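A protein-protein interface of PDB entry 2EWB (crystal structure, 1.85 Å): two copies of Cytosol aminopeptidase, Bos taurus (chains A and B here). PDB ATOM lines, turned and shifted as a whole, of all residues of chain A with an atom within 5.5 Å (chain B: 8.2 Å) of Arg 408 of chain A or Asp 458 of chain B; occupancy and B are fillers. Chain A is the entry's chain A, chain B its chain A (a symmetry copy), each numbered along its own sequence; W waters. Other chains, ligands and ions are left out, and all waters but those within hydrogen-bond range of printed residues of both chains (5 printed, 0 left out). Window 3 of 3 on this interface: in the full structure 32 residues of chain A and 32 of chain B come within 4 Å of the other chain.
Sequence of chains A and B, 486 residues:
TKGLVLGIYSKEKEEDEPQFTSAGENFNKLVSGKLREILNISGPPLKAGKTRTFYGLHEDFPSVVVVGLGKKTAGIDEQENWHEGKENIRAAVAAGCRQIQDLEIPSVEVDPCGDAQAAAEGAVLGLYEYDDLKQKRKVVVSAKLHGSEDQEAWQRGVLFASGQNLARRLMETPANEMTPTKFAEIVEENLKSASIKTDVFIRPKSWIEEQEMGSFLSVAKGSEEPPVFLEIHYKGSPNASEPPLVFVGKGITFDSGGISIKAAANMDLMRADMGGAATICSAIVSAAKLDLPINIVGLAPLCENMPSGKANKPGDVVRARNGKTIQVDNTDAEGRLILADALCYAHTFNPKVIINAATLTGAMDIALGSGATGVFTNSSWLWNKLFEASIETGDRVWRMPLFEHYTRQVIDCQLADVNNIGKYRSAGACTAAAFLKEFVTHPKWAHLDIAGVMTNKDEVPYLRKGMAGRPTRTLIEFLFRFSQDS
OG of Ser 370 of chain B lies within hydrogen-bond range of OE2 of Glu 459 of chain B, 2.6 Å away. The backbone NH of Lys 457 of chain B is in hydrogen-bond range of the side-chain carboxylate of Glu 459 of chain B, at 2.7 Å. O of Gln 409 of chain A sits at hydrogen-bond distance from N of Lys 423 of chain A, at 3.1 Å. OD2 of Asp 412 of chain A lies within salt-bridge range of NZ of Lys 423 of chain A (3.7 Å). The side-chain carboxylate of Glu 459 of chain B lies close to the side-chain amide oxygen of Asn 456 of chain B (3.4 Å).
His 405 of chain A touches Glu 459 of chain B (NE2 to CB, 3.5 Å). NH1 of Arg 408 of chain A touches O of Glu 459 of chain B, 3.9 Å away. CG of Glu 459 of chain B touches OE1 of Gln 409 of chain A, at 3.96 Å. Tyr 424 of chain A touches Lys 457 of chain B.
Hydrophobic or aromatic side chains of chain A that line the printed part of chain B: His 405 and Tyr 424. Of the 13 printed residues of chain B, 4 touch a printed residue of chain A. Among the printed residues, 8 pairs touch across the chains.
Arg 408 of chain A touches just these residues of chain B: Asp 458 and Glu 459. Of chain A, only Arg 408 (2.8 Å), Lys 423 (3.5 Å) and Tyr 424 (2.9 Å) come within 4 Å of Asp 458 of chain B. Printed residues of chain B within 4 Å of Lys 423 of chain A: Asp 458. Printed residues of chain B within 4 Å of His 405 of chain A: Ser 370 (3.0 Å) and Glu 459 (3.5 Å). Of the printed residues of chain A, Ser 370 of chain B touches His 405 (3.0 Å). Gly 466 of chain B touches none of the printed residues of chain A. The nearest residue of chain B that does not touch Arg 408 of chain A is Pro 461 of chain B (5.1 Å). The nearest printed residue of chain A that does not touch Asp 458 of chain B is Gln 409 of chain A (6.1 Å). The nearest printed residue of chain B that does not touch Tyr 424 of chain A is Glu 459 of chain B (4.5 Å).
The side-chain carboxylate (OD1) of Asp 458 of chain B sits at hydrogen-bond distance from the side-chain hydroxyl (OH) of Tyr 424 of chain A (2.9 Å). The side-chain carboxylate (OD2) of Asp 458 of chain B lies within salt-bridge range of the guanidinium group (NH2) of Arg 408 of chain A (2.8 Å). OD2 of Asp 458 of chain B lies within salt-bridge range of NZ of Lys 423 of chain A, at 3.5 Å. A ring nitrogen (NE2) of His 405 of chain A lies within hydrogen-bond range of the side-chain hydroxyl of Ser 370 of chain B (3.0 Å).
No position is printed for both chains. Of the 8 pairs that touch across the chains among the printed residues, none has its exchanged pair printed and touching as well.
Water W5 lies within hydrogen-bond range of the side-chain carboxylate (OE2) of Glu 459 of chain B (2.7 Å), the side-chain amide oxygen (OE1) of Gln 409 of chain A (3.2 Å) and the side-chain hydroxyl (OG) of Ser 370 of chain B (3.4 Å). Water W4 bridges O of Asp 458 of chain B (2.7 Å) and NH2 of Arg 408 of chain A (3.2 Å). Water W1 lies within hydrogen-bond range of the backbone carbonyl oxygen (O) of Glu 459 of chain B and the guanidinium group (NH1) of Arg 408 of chain A. Water W3 lies within hydrogen-bond range of the backbone NH (N) of Ser 370 of chain B (3.0 Å) and the side-chain amide oxygen (OE1) of Gln 409 of chain A (3.5 Å). Water W2 lies within hydrogen-bond range of the side-chain carboxylate (OD1) of Asp 458 of chain B and the side-chain amino group (NZ) of Lys 423 of chain A.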
ATOM      1  N   GLU A 404      15.012 -14.876  20.722  1.00  0.00           N
ATOM      2  CA  GLU A 404      14.517 -13.734  19.963  1.00  0.00           C
ATOM      3  C   GLU A 404      15.476 -12.569  20.218  1.00  0.00           C
ATOM      4  O   GLU A 404      15.582 -11.639  19.420  1.00  0.00           O
ATOM      5  CB  GLU A 404      13.099 -13.383  20.423  1.00  0.00           C
ATOM      6  CG  GLU A 404      12.459 -12.183  19.734  1.00  0.00           C
ATOM      7  CD  GLU A 404      12.946 -10.853  20.280  1.00  0.00           C
ATOM      8  OE1 GLU A 404      13.338 -10.803  21.464  1.00  0.00           O
ATOM      9  OE2 GLU A 404      12.918  -9.852  19.532  1.00  0.00           O
ATOM     10  N   HIS A 405      16.172 -12.645  21.348  1.00  0.00           N
ATOM     11  CA  HIS A 405      17.159 -11.642  21.748  1.00  0.00           C
ATOM     12  C   HIS A 405      18.104 -11.391  20.569  1.00  0.00           C
ATOM     13  O   HIS A 405      18.412 -10.246  20.225  1.00  0.00           O
ATOM     14  CB  HIS A 405      17.916 -12.184  22.971  1.00  0.00           C
ATOM     15  CG  HIS A 405      19.080 -11.351  23.412  1.00  0.00           C
ATOM     16  ND1 HIS A 405      20.230 -11.213  22.664  1.00  0.00           N
ATOM     17  CD2 HIS A 405      19.308 -10.689  24.572  1.00  0.00           C
ATOM     18  CE1 HIS A 405      21.115 -10.507  23.346  1.00  0.00           C
ATOM     19  NE2 HIS A 405      20.579 -10.177  24.508  1.00  0.00           N
ATOM     20  N   TYR A 406      18.544 -12.473  19.937  1.00  0.00           N
ATOM     21  CA  TYR A 406      19.455 -12.370  18.802  1.00  0.00           C
ATOM     22  C   TYR A 406      18.722 -11.983  17.522  1.00  0.00           C
ATOM     23  O   TYR A 406      19.247 -11.228  16.706  1.00  0.00           O
ATOM     24  CB  TYR A 406      20.196 -13.694  18.619  1.00  0.00           C
ATOM     25  CG  TYR A 406      20.901 -14.137  19.881  1.00  0.00           C
ATOM     26  CD1 TYR A 406      21.978 -13.412  20.393  1.00  0.00           C
ATOM     27  CD2 TYR A 406      20.468 -15.258  20.585  1.00  0.00           C
ATOM     28  CE1 TYR A 406      22.607 -13.793  21.577  1.00  0.00           C
ATOM     29  CE2 TYR A 406      21.087 -15.648  21.774  1.00  0.00           C
ATOM     30  CZ  TYR A 406      22.154 -14.911  22.262  1.00  0.00           C
ATOM     31  OH  TYR A 406      22.767 -15.289  23.435  1.00  0.00           O
ATOM     32  N   THR A 407      17.509 -12.498  17.351  1.00  0.00           N
ATOM     33  CA  THR A 407      16.704 -12.191  16.172  1.00  0.00           C
ATOM     34  C   THR A 407      16.522 -10.683  16.046  1.00  0.00           C
ATOM     35  O   THR A 407      16.662 -10.110  14.968  1.00  0.00           O
ATOM     36  CB  THR A 407      15.308 -12.831  16.272  1.00  0.00           C
ATOM     37  OG1 THR A 407      15.436 -14.256  16.327  1.00  0.00           O
ATOM     38  CG2 THR A 407      14.454 -12.439  15.078  1.00  0.00           C
ATOM     39  N   ARG A 408      16.208 -10.051  17.168  1.00  0.00           N
ATOM     40  CA  ARG A 408      15.986  -8.617  17.210  1.00  0.00           C
ATOM     41  C   ARG A 408      17.168  -7.842  16.636  1.00  0.00           C
ATOM     42  O   ARG A 408      16.993  -6.794  16.018  1.00  0.00           O
ATOM     43  CB  ARG A 408      15.742  -8.184  18.657  1.00  0.00           C
ATOM     44  CG  ARG A 408      15.392  -6.722  18.817  1.00  0.00           C
ATOM     45  CD  ARG A 408      15.309  -6.356  20.287  1.00  0.00           C
ATOM     46  NE  ARG A 408      15.075  -4.929  20.482  1.00  0.00           N
ATOM     47  CZ  ARG A 408      15.157  -4.317  21.658  1.00  0.00           C
ATOM     48  NH1 ARG A 408      15.469  -5.011  22.744  1.00  0.00           N
ATOM     49  NH2 ARG A 408      14.932  -3.012  21.746  1.00  0.00           N
ATOM     50  N   GLN A 409      18.370  -8.370  16.832  1.00  0.00           N
ATOM     51  CA  GLN A 409      19.569  -7.701  16.356  1.00  0.00           C
ATOM     52  C   GLN A 409      19.829  -7.840  14.860  1.00  0.00           C
ATOM     53  O   GLN A 409      20.656  -7.116  14.306  1.00  0.00           O
ATOM     54  CB  GLN A 409      20.768  -8.178  17.177  1.00  0.00           C
ATOM     55  CG  GLN A 409      20.576  -7.874  18.662  1.00  0.00           C
ATOM     56  CD  GLN A 409      21.756  -8.259  19.525  1.00  0.00           C
ATOM     57  OE1 GLN A 409      21.675  -8.218  20.755  1.00  0.00           O
ATOM     58  NE2 GLN A 409      22.857  -8.628  18.896  1.00  0.00           N
ATOM     59  N   VAL A 410      19.126  -8.756  14.200  1.00  0.00           N
ATOM     60  CA  VAL A 410      19.302  -8.915  12.763  1.00  0.00           C
ATOM     61  C   VAL A 410      18.104  -8.373  11.992  1.00  0.00           C
ATOM     62  O   VAL A 410      18.225  -8.039  10.815  1.00  0.00           O
ATOM     63  CB  VAL A 410      19.545 -10.387  12.361  1.00  0.00           C
ATOM     64  CG1 VAL A 410      20.848 -10.876  12.975  1.00  0.00           C
ATOM     65  CG2 VAL A 410      18.378 -11.256  12.798  1.00  0.00           C
ATOM     66  N   ILE A 411      16.943  -8.288  12.639  1.00  0.00           N
ATOM     67  CA  ILE A 411      15.785  -7.743  11.945  1.00  0.00           C
ATOM     68  C   ILE A 411      15.741  -6.231  12.125  1.00  0.00           C
ATOM     69  O   ILE A 411      14.914  -5.549  11.525  1.00  0.00           O
ATOM     70  CB  ILE A 411      14.448  -8.378  12.402  1.00  0.00           C
ATOM     71  CG1 ILE A 411      14.244  -8.195  13.900  1.00  0.00           C
ATOM     72  CG2 ILE A 411      14.426  -9.847  12.017  1.00  0.00           C
ATOM     73  CD1 ILE A 411      12.885  -8.686  14.367  1.00  0.00           C
ATOM     74  N   ASP A 412      16.624  -5.710  12.970  1.00  0.00           N
ATOM     75  CA  ASP A 412      16.717  -4.267  13.140  1.00  0.00           C
ATOM     76  C   ASP A 412      17.566  -3.949  11.918  1.00  0.00           C
ATOM     77  O   ASP A 412      18.797  -3.968  11.974  1.00  0.00           O
ATOM     78  CB  ASP A 412      17.466  -3.908  14.425  1.00  0.00           C
ATOM     79  CG  ASP A 412      17.581  -2.411  14.626  1.00  0.00           C
ATOM     80  OD1 ASP A 412      16.582  -1.704  14.369  1.00  0.00           O
ATOM     81  OD2 ASP A 412      18.658  -1.943  15.048  1.00  0.00           O
ATOM     82  N   LYS A 423      23.537  -6.038  14.630  1.00  0.00           N
ATOM     83  CA  LYS A 423      23.856  -4.636  14.855  1.00  0.00           C
ATOM     84  C   LYS A 423      25.006  -4.501  15.843  1.00  0.00           C
ATOM     85  O   LYS A 423      25.669  -3.466  15.897  1.00  0.00           O
ATOM     86  CB  LYS A 423      22.625  -3.868  15.349  1.00  0.00           C
ATOM     87  CG  LYS A 423      21.960  -4.424  16.588  1.00  0.00           C
ATOM     88  CD  LYS A 423      20.769  -3.553  16.968  1.00  0.00           C
ATOM     89  CE  LYS A 423      20.025  -4.107  18.171  1.00  0.00           C
ATOM     90  NZ  LYS A 423      18.875  -3.236  18.559  1.00  0.00           N
ATOM     91  N   TYR A 424      25.236  -5.555  16.619  1.00  0.00           N
ATOM     92  CA  TYR A 424      26.328  -5.577  17.584  1.00  0.00           C
ATOM     93  C   TYR A 424      27.272  -6.697  17.144  1.00  0.00           C
ATOM     94  O   TYR A 424      26.880  -7.590  16.393  1.00  0.00           O
ATOM     95  CB  TYR A 424      25.803  -5.853  19.000  1.00  0.00           C
ATOM     96  CG  TYR A 424      24.711  -4.907  19.467  1.00  0.00           C
ATOM     97  CD1 TYR A 424      24.846  -3.524  19.331  1.00  0.00           C
ATOM     98  CD2 TYR A 424      23.546  -5.398  20.058  1.00  0.00           C
ATOM     99  CE1 TYR A 424      23.848  -2.652  19.772  1.00  0.00           C
ATOM    100  CE2 TYR A 424      22.541  -4.536  20.504  1.00  0.00           C
ATOM    101  CZ  TYR A 424      22.698  -3.165  20.356  1.00  0.00           C
ATOM    102  OH  TYR A 424      21.704  -2.313  20.787  1.00  0.00           O
ATOM    103  N   SER B 370      24.892 -10.730  25.421  1.00  0.00           N
ATOM    104  CA  SER B 370      24.120 -10.472  26.630  1.00  0.00           C
ATOM    105  C   SER B 370      22.877 -11.354  26.710  1.00  0.00           C
ATOM    106  O   SER B 370      22.011 -11.146  27.562  1.00  0.00           O
ATOM    107  CB  SER B 370      23.708  -8.999  26.684  1.00  0.00           C
ATOM    108  OG  SER B 370      22.968  -8.642  25.533  1.00  0.00           O
ATOM    109  N   THR B 455      27.062  -5.403  30.548  1.00  0.00           N
ATOM    110  CA  THR B 455      26.339  -4.182  30.226  1.00  0.00           C
ATOM    111  C   THR B 455      25.019  -4.449  29.534  1.00  0.00           C
ATOM    112  O   THR B 455      24.720  -5.572  29.120  1.00  0.00           O
ATOM    113  CB  THR B 455      27.145  -3.287  29.271  1.00  0.00           C
ATOM    114  OG1 THR B 455      27.206  -3.914  27.981  1.00  0.00           O
ATOM    115  CG2 THR B 455      28.558  -3.076  29.789  1.00  0.00           C
ATOM    116  N   ASN B 456      24.228  -3.393  29.414  1.00  0.00           N
ATOM    117  CA  ASN B 456      22.962  -3.469  28.719  1.00  0.00           C
ATOM    118  C   ASN B 456      22.844  -2.213  27.890  1.00  0.00           C
ATOM    119  O   ASN B 456      23.226  -1.126  28.328  1.00  0.00           O
ATOM    120  CB  ASN B 456      21.777  -3.531  29.685  1.00  0.00           C
ATOM    121  CG  ASN B 456      20.476  -3.883  28.979  1.00  0.00           C
ATOM    122  OD1 ASN B 456      20.344  -4.969  28.430  1.00  0.00           O
ATOM    123  ND2 ASN B 456      19.513  -2.960  28.987  1.00  0.00           N
ATOM    124  N   LYS B 457      22.351  -2.374  26.673  1.00  0.00           N
ATOM    125  CA  LYS B 457      22.119  -1.244  25.799  1.00  0.00           C
ATOM    126  C   LYS B 457      20.603  -1.161  25.800  1.00  0.00           C
ATOM    127  O   LYS B 457      20.025  -0.260  26.405  1.00  0.00           O
ATOM    128  CB  LYS B 457      22.667  -1.537  24.402  1.00  0.00           C
ATOM    129  CG  LYS B 457      24.182  -1.623  24.387  1.00  0.00           C
ATOM    130  CD  LYS B 457      24.680  -2.658  23.399  1.00  0.00           C
ATOM    131  CE  LYS B 457      26.122  -3.009  23.692  1.00  0.00           C
ATOM    132  NZ  LYS B 457      26.581  -4.156  22.877  1.00  0.00           N
ATOM    133  N   ASP B 458      19.966  -2.142  25.170  1.00  0.00           N
ATOM    134  CA  ASP B 458      18.512  -2.189  25.107  1.00  0.00           C
ATOM    135  C   ASP B 458      18.002  -3.629  25.069  1.00  0.00           C
ATOM    136  O   ASP B 458      16.804  -3.855  24.926  1.00  0.00           O
ATOM    137  CB  ASP B 458      18.028  -1.449  23.858  1.00  0.00           C
ATOM    138  CG  ASP B 458      18.372  -2.183  22.576  1.00  0.00           C
ATOM    139  OD1 ASP B 458      19.422  -2.864  22.529  1.00  0.00           O
ATOM    140  OD2 ASP B 458      17.596  -2.072  21.604  1.00  0.00           O
ATOM    141  N   GLU B 459      18.904  -4.598  25.208  1.00  0.00           N
ATOM    142  CA  GLU B 459      18.520  -6.010  25.145  1.00  0.00           C
ATOM    143  C   GLU B 459      17.503  -6.393  26.205  1.00  0.00           C
ATOM    144  O   GLU B 459      16.497  -7.039  25.904  1.00  0.00           O
ATOM    145  CB  GLU B 459      19.748  -6.910  25.270  1.00  0.00           C
ATOM    146  CG  GLU B 459      20.834  -6.597  24.266  1.00  0.00           C
ATOM    147  CD  GLU B 459      21.910  -5.706  24.846  1.00  0.00           C
ATOM    148  OE1 GLU B 459      21.589  -4.581  25.291  1.00  0.00           O
ATOM    149  OE2 GLU B 459      23.080  -6.141  24.860  1.00  0.00           O
ATOM    150  N   VAL B 460      17.786  -6.025  27.450  1.00  0.00           N
ATOM    151  CA  VAL B 460      16.861  -6.291  28.543  1.00  0.00           C
ATOM    152  C   VAL B 460      16.086  -4.984  28.631  1.00  0.00           C
ATOM    153  O   VAL B 460      16.628  -3.959  29.037  1.00  0.00           O
ATOM    154  CB  VAL B 460      17.599  -6.560  29.864  1.00  0.00           C
ATOM    155  CG1 VAL B 460      16.593  -6.867  30.957  1.00  0.00           C
ATOM    156  CG2 VAL B 460      18.569  -7.728  29.689  1.00  0.00           C
ATOM    157  N   PRO B 461      14.809  -5.004  28.230  1.00  0.00           N
ATOM    158  CA  PRO B 461      13.920  -3.838  28.229  1.00  0.00           C
ATOM    159  C   PRO B 461      13.848  -3.049  29.526  1.00  0.00           C
ATOM    160  O   PRO B 461      13.805  -1.817  29.507  1.00  0.00           O
ATOM    161  CB  PRO B 461      12.562  -4.436  27.861  1.00  0.00           C
ATOM    162  CG  PRO B 461      12.918  -5.647  27.062  1.00  0.00           C
ATOM    163  CD  PRO B 461      14.068  -6.219  27.845  1.00  0.00           C
ATOM    164  N   TYR B 462      13.835  -3.757  30.648  1.00  0.00           N
ATOM    165  CA  TYR B 462      13.722  -3.107  31.944  1.00  0.00           C
ATOM    166  C   TYR B 462      15.024  -2.645  32.584  1.00  0.00           C
ATOM    167  O   TYR B 462      15.066  -2.344  33.777  1.00  0.00           O
ATOM    168  CB  TYR B 462      12.942  -4.012  32.903  1.00  0.00           C
ATOM    169  CG  TYR B 462      13.427  -5.440  32.954  1.00  0.00           C
ATOM    170  CD1 TYR B 462      14.429  -5.825  33.843  1.00  0.00           C
ATOM    171  CD2 TYR B 462      12.858  -6.416  32.137  1.00  0.00           C
ATOM    172  CE1 TYR B 462      14.847  -7.152  33.924  1.00  0.00           C
ATOM    173  CE2 TYR B 462      13.268  -7.744  32.209  1.00  0.00           C
ATOM    174  CZ  TYR B 462      14.259  -8.105  33.104  1.00  0.00           C
ATOM    175  OH  TYR B 462      14.646  -9.421  33.191  1.00  0.00           O
ATOM    176  N   LEU B 463      16.088  -2.594  31.793  1.00  0.00           N
ATOM    177  CA  LEU B 463      17.368  -2.109  32.288  1.00  0.00           C
ATOM    178  C   LEU B 463      17.807  -0.978  31.372  1.00  0.00           C
ATOM    179  O   LEU B 463      17.924  -1.162  30.162  1.00  0.00           O
ATOM    180  CB  LEU B 463      18.432  -3.210  32.272  1.00  0.00           C
ATOM    181  CG  LEU B 463      18.204  -4.442  33.144  1.00  0.00           C
ATOM    182  CD1 LEU B 463      19.358  -5.418  32.945  1.00  0.00           C
ATOM    183  CD2 LEU B 463      18.090  -4.028  34.606  1.00  0.00           C
ATOM    184  N   ARG B 464      18.030   0.198  31.942  1.00  0.00           N
ATOM    185  CA  ARG B 464      18.482   1.327  31.144  1.00  0.00           C
ATOM    186  C   ARG B 464      19.926   1.059  30.726  1.00  0.00           C
ATOM    187  O   ARG B 464      20.579   0.167  31.270  1.00  0.00           O
ATOM    188  CB  ARG B 464      18.375   2.618  31.956  1.00  0.00           C
ATOM    189  CG  ARG B 464      16.963   3.185  31.960  1.00  0.00           C
ATOM    190  CD  ARG B 464      16.800   4.351  32.916  1.00  0.00           C
ATOM    191  NE  ARG B 464      15.702   5.222  32.503  1.00  0.00           N
ATOM    192  CZ  ARG B 464      14.953   5.933  33.340  1.00  0.00           C
ATOM    193  NH1 ARG B 464      15.176   5.875  34.645  1.00  0.00           N
ATOM    194  NH2 ARG B 464      13.987   6.711  32.868  1.00  0.00           N
ATOM    195  N   LYS B 465      20.418   1.816  29.755  1.00  0.00           N
ATOM    196  CA  LYS B 465      21.782   1.643  29.272  1.00  0.00           C
ATOM    197  C   LYS B 465      22.790   1.785  30.410  1.00  0.00           C
ATOM    198  O   LYS B 465      22.733   2.735  31.186  1.00  0.00           O
ATOM    199  CB  LYS B 465      22.090   2.675  28.183  1.00  0.00           C
ATOM    200  CG  LYS B 465      23.510   2.602  27.644  1.00  0.00           C
ATOM    201  CD  LYS B 465      23.759   3.683  26.602  1.00  0.00           C
ATOM    202  CE  LYS B 465      25.186   3.631  26.068  1.00  0.00           C
ATOM    203  NZ  LYS B 465      25.453   4.738  25.104  1.00  0.00           N
ATOM    204  N   GLY B 466      23.714   0.837  30.501  1.00  0.00           N
ATOM    205  CA  GLY B 466      24.715   0.890  31.550  1.00  0.00           C
ATOM    206  C   GLY B 466      25.029  -0.493  32.084  1.00  0.00           C
ATOM    207  O   GLY B 466      24.604  -1.493  31.504  1.00  0.00           O
HETATM  208  O   HOH W   1      16.303  -7.794  23.277  1.00  0.00           O
HETATM  209  O   HOH W   2      19.010  -5.479  20.875  1.00  0.00           O
HETATM  210  O   HOH W   3      23.896  -9.968  22.732  1.00  0.00           O
HETATM  211  O   HOH W   4      14.367  -2.641  24.844  1.00  0.00           O
HETATM  212  O   HOH W   5      24.106  -7.255  22.661  1.00  0.00           O
